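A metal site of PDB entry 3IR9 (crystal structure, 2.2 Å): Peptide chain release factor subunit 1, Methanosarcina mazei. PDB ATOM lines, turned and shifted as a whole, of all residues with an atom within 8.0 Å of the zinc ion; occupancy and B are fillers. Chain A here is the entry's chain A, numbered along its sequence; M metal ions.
The side-chain sulfur (SG) of Cys 81 lies close to the backbone NH (N) of Val 83 (3.7 Å).
The backbone carbonyl oxygen (O) of Tyr 86 is in hydrogen-bond range of the backbone NH (N) of Cys 81, 2.9 Å away.
The backbone NH of Lys 108 sits close to the side-chain sulfur of Cys 106, 3.6 Å away.
The side-chain sulfur (SG) of Cys 84 lies close to the backbone NH (N) of Tyr 86 (3.4 Å).
N of Cys 106 lies within hydrogen-bond range of O of Ser 111, at 2.5 Å.
SG of Cys 109 sits close to OG of Ser 111 (3.1 Å).
Within 4 Å of the zinc ion: Cys 81, Cys 84, Cys 106 and Cys 109.
SG of Cys 109 binds the zinc ion (2.3 Å).
The zinc ion is bound by the side-chain sulfur (SG) of Cys 106, at 2.3 Å.
The zinc ion is bound by SG of Cys 81, at 2.4 Å.
The zinc ion is bound by SG of Cys 84, at 2.6 Å.
The zinc ion has four donor atoms within binding distance.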
ATOM      1  N   LYS A  80      15.559  24.662  29.391  1.00  0.00           N
ATOM      2  CA  LYS A  80      15.877  23.383  28.764  1.00  0.00           C
ATOM      3  C   LYS A  80      15.046  22.228  29.342  1.00  0.00           C
ATOM      4  O   LYS A  80      14.762  22.185  30.538  1.00  0.00           O
ATOM      5  CB  LYS A  80      17.373  23.092  28.896  1.00  0.00           C
ATOM      6  CG  LYS A  80      18.279  24.182  28.380  1.00  0.00           C
ATOM      7  CD  LYS A  80      19.725  23.811  28.579  1.00  0.00           C
ATOM      8  CE  LYS A  80      20.633  25.010  28.428  1.00  0.00           C
ATOM      9  NZ  LYS A  80      22.015  24.715  28.908  1.00  0.00           N
ATOM     10  N   CYS A  81      14.662  21.301  28.480  1.00  0.00           N
ATOM     11  CA  CYS A  81      13.849  20.173  28.919  1.00  0.00           C
ATOM     12  C   CYS A  81      14.672  19.178  29.715  1.00  0.00           C
ATOM     13  O   CYS A  81      15.820  18.888  29.387  1.00  0.00           O
ATOM     14  CB  CYS A  81      13.174  19.487  27.732  1.00  0.00           C
ATOM     15  SG  CYS A  81      12.069  18.174  28.230  1.00  0.00           S
ATOM     16  N   SER A  82      14.059  18.656  30.768  1.00  0.00           N
ATOM     17  CA  SER A  82      14.742  17.793  31.719  1.00  0.00           C
ATOM     18  C   SER A  82      14.990  16.372  31.197  1.00  0.00           C
ATOM     19  O   SER A  82      15.681  15.590  31.847  1.00  0.00           O
ATOM     20  CB  SER A  82      13.950  17.751  33.023  1.00  0.00           C
ATOM     21  OG  SER A  82      12.571  17.565  32.779  1.00  0.00           O
ATOM     22  N   VAL A  83      14.421  16.042  30.036  1.00  0.00           N
ATOM     23  CA  VAL A  83      14.636  14.714  29.457  1.00  0.00           C
ATOM     24  C   VAL A  83      15.091  14.754  27.991  1.00  0.00           C
ATOM     25  O   VAL A  83      16.139  14.220  27.655  1.00  0.00           O
ATOM     26  CB  VAL A  83      13.400  13.779  29.633  1.00  0.00           C
ATOM     27  CG1 VAL A  83      12.807  13.951  31.025  1.00  0.00           C
ATOM     28  CG2 VAL A  83      12.353  14.050  28.577  1.00  0.00           C
ATOM     29  N   CYS A  84      14.298  15.376  27.125  1.00  0.00           N
ATOM     30  CA  CYS A  84      14.647  15.424  25.720  1.00  0.00           C
ATOM     31  C   CYS A  84      15.506  16.644  25.423  1.00  0.00           C
ATOM     32  O   CYS A  84      15.846  17.415  26.325  1.00  0.00           O
ATOM     33  CB  CYS A  84      13.388  15.326  24.819  1.00  0.00           C
ATOM     34  SG  CYS A  84      12.616  16.872  24.284  1.00  0.00           S
ATOM     35  N   GLY A  85      15.882  16.810  24.158  1.00  0.00           N
ATOM     36  CA  GLY A  85      16.804  17.860  23.775  1.00  0.00           C
ATOM     37  C   GLY A  85      16.154  19.206  23.534  1.00  0.00           C
ATOM     38  O   GLY A  85      16.766  20.095  22.950  1.00  0.00           O
ATOM     39  N   TYR A  86      14.919  19.375  23.983  1.00  0.00           N
ATOM     40  CA  TYR A  86      14.231  20.649  23.769  1.00  0.00           C
ATOM     41  C   TYR A  86      14.896  21.797  24.551  1.00  0.00           C
ATOM     42  O   TYR A  86      15.332  21.611  25.692  1.00  0.00           O
ATOM     43  CB  TYR A  86      12.742  20.562  24.134  1.00  0.00           C
ATOM     44  CG  TYR A  86      12.017  21.872  23.921  1.00  0.00           C
ATOM     45  CD1 TYR A  86      11.672  22.299  22.647  1.00  0.00           C
ATOM     46  CD2 TYR A  86      11.717  22.708  24.997  1.00  0.00           C
ATOM     47  CE1 TYR A  86      11.025  23.510  22.446  1.00  0.00           C
ATOM     48  CE2 TYR A  86      11.064  23.927  24.799  1.00  0.00           C
ATOM     49  CZ  TYR A  86      10.728  24.324  23.516  1.00  0.00           C
ATOM     50  OH  TYR A  86      10.078  25.522  23.313  1.00  0.00           O
ATOM     51  N   GLU A  87      14.973  22.964  23.917  1.00  0.00           N
ATOM     52  CA  GLU A  87      15.415  24.186  24.599  1.00  0.00           C
ATOM     53  C   GLU A  87      14.842  25.422  23.925  1.00  0.00           C
ATOM     54  O   GLU A  87      14.432  25.394  22.763  1.00  0.00           O
ATOM     55  CB  GLU A  87      16.945  24.283  24.646  1.00  0.00           C
ATOM     56  CG  GLU A  87      17.543  25.170  23.557  1.00  0.00           C
ATOM     57  CD  GLU A  87      19.054  25.275  23.617  1.00  0.00           C
ATOM     58  OE1 GLU A  87      19.610  26.244  23.056  1.00  0.00           O
ATOM     59  OE2 GLU A  87      19.701  24.386  24.225  1.00  0.00           O
ATOM     60  N   ASN A 105       5.888  23.070  30.883  1.00  0.00           N
ATOM     61  CA  ASN A 105       6.100  21.728  30.301  1.00  0.00           C
ATOM     62  C   ASN A 105       6.701  21.742  28.890  1.00  0.00           C
ATOM     63  O   ASN A 105       6.646  22.740  28.173  1.00  0.00           O
ATOM     64  CB  ASN A 105       4.799  20.934  30.267  1.00  0.00           C
ATOM     65  CG  ASN A 105       4.346  20.492  31.647  1.00  0.00           C
ATOM     66  OD1 ASN A 105       5.150  20.259  32.544  1.00  0.00           O
ATOM     67  ND2 ASN A 105       3.028  20.357  31.813  1.00  0.00           N
ATOM     68  N   CYS A 106       7.241  20.590  28.494  1.00  0.00           N
ATOM     69  CA  CYS A 106       7.884  20.441  27.186  1.00  0.00           C
ATOM     70  C   CYS A 106       6.864  20.234  26.066  1.00  0.00           C
ATOM     71  O   CYS A 106       6.116  19.264  26.075  1.00  0.00           O
ATOM     72  CB  CYS A 106       8.871  19.268  27.217  1.00  0.00           C
ATOM     73  SG  CYS A 106      10.023  19.204  25.810  1.00  0.00           S
ATOM     74  N   PRO A 107       6.852  21.149  25.090  1.00  0.00           N
ATOM     75  CA  PRO A 107       5.895  21.044  23.990  1.00  0.00           C
ATOM     76  C   PRO A 107       6.288  19.890  23.068  1.00  0.00           C
ATOM     77  O   PRO A 107       5.597  19.607  22.103  1.00  0.00           O
ATOM     78  CB  PRO A 107       6.036  22.392  23.281  1.00  0.00           C
ATOM     79  CG  PRO A 107       6.752  23.279  24.265  1.00  0.00           C
ATOM     80  CD  PRO A 107       7.668  22.369  24.992  1.00  0.00           C
ATOM     81  N   LYS A 108       7.397  19.231  23.398  1.00  0.00           N
ATOM     82  CA  LYS A 108       7.887  18.096  22.608  1.00  0.00           C
ATOM     83  C   LYS A 108       7.566  16.751  23.259  1.00  0.00           C
ATOM     84  O   LYS A 108       7.030  15.862  22.591  1.00  0.00           O
ATOM     85  CB  LYS A 108       9.399  18.220  22.385  1.00  0.00           C
ATOM     86  CG  LYS A 108       9.759  19.225  21.310  1.00  0.00           C
ATOM     87  CD  LYS A 108       9.279  18.736  19.960  1.00  0.00           C
ATOM     88  CE  LYS A 108       9.334  19.845  18.912  1.00  0.00           C
ATOM     89  NZ  LYS A 108       8.544  19.473  17.705  1.00  0.00           N
ATOM     90  N   CYS A 109       7.880  16.602  24.540  1.00  0.00           N
ATOM     91  CA  CYS A 109       7.710  15.316  25.225  1.00  0.00           C
ATOM     92  C   CYS A 109       6.830  15.429  26.470  1.00  0.00           C
ATOM     93  O   CYS A 109       6.541  14.429  27.138  1.00  0.00           O
ATOM     94  CB  CYS A 109       9.063  14.735  25.618  1.00  0.00           C
ATOM     95  SG  CYS A 109       9.717  15.409  27.143  1.00  0.00           S
ATOM     96  N   GLY A 110       6.409  16.652  26.781  1.00  0.00           N
ATOM     97  CA  GLY A 110       5.526  16.876  27.898  1.00  0.00           C
ATOM     98  C   GLY A 110       6.179  16.840  29.264  1.00  0.00           C
ATOM     99  O   GLY A 110       5.477  16.919  30.282  1.00  0.00           O
ATOM    100  N   SER A 111       7.500  16.726  29.317  1.00  0.00           N
ATOM    101  CA  SER A 111       8.218  16.751  30.590  1.00  0.00           C
ATOM    102  C   SER A 111       8.360  18.185  31.107  1.00  0.00           C
ATOM    103  O   SER A 111       8.206  19.139  30.346  1.00  0.00           O
ATOM    104  CB  SER A 111       9.603  16.122  30.444  1.00  0.00           C
ATOM    105  OG  SER A 111       9.493  14.757  30.116  1.00  0.00           O
ATOM    106  N   SER A 112       8.673  18.322  32.395  1.00  0.00           N
ATOM    107  CA  SER A 112       8.854  19.638  32.984  1.00  0.00           C
ATOM    108  C   SER A 112      10.115  20.314  32.457  1.00  0.00           C
ATOM    109  O   SER A 112      11.208  19.750  32.512  1.00  0.00           O
ATOM    110  CB  SER A 112       8.904  19.557  34.517  1.00  0.00           C
ATOM    111  OG  SER A 112       8.878  20.838  35.113  1.00  0.00           O
ATOM    112  N   LEU A 113       9.949  21.522  31.922  1.00  0.00           N
ATOM    113  CA  LEU A 113      11.079  22.365  31.588  1.00  0.00           C
ATOM    114  C   LEU A 113      11.643  22.971  32.867  1.00  0.00           C
ATOM    115  O   LEU A 113      10.997  22.927  33.923  1.00  0.00           O
ATOM    116  CB  LEU A 113      10.640  23.477  30.627  1.00  0.00           C
ATOM    117  CG  LEU A 113       9.995  23.012  29.316  1.00  0.00           C
ATOM    118  CD1 LEU A 113       9.378  24.197  28.581  1.00  0.00           C
ATOM    119  CD2 LEU A 113      11.002  22.307  28.426  1.00  0.00           C
HETATM  120 ZN    ZN M   1      10.996  17.149  26.332  1.00  0.00          ZN
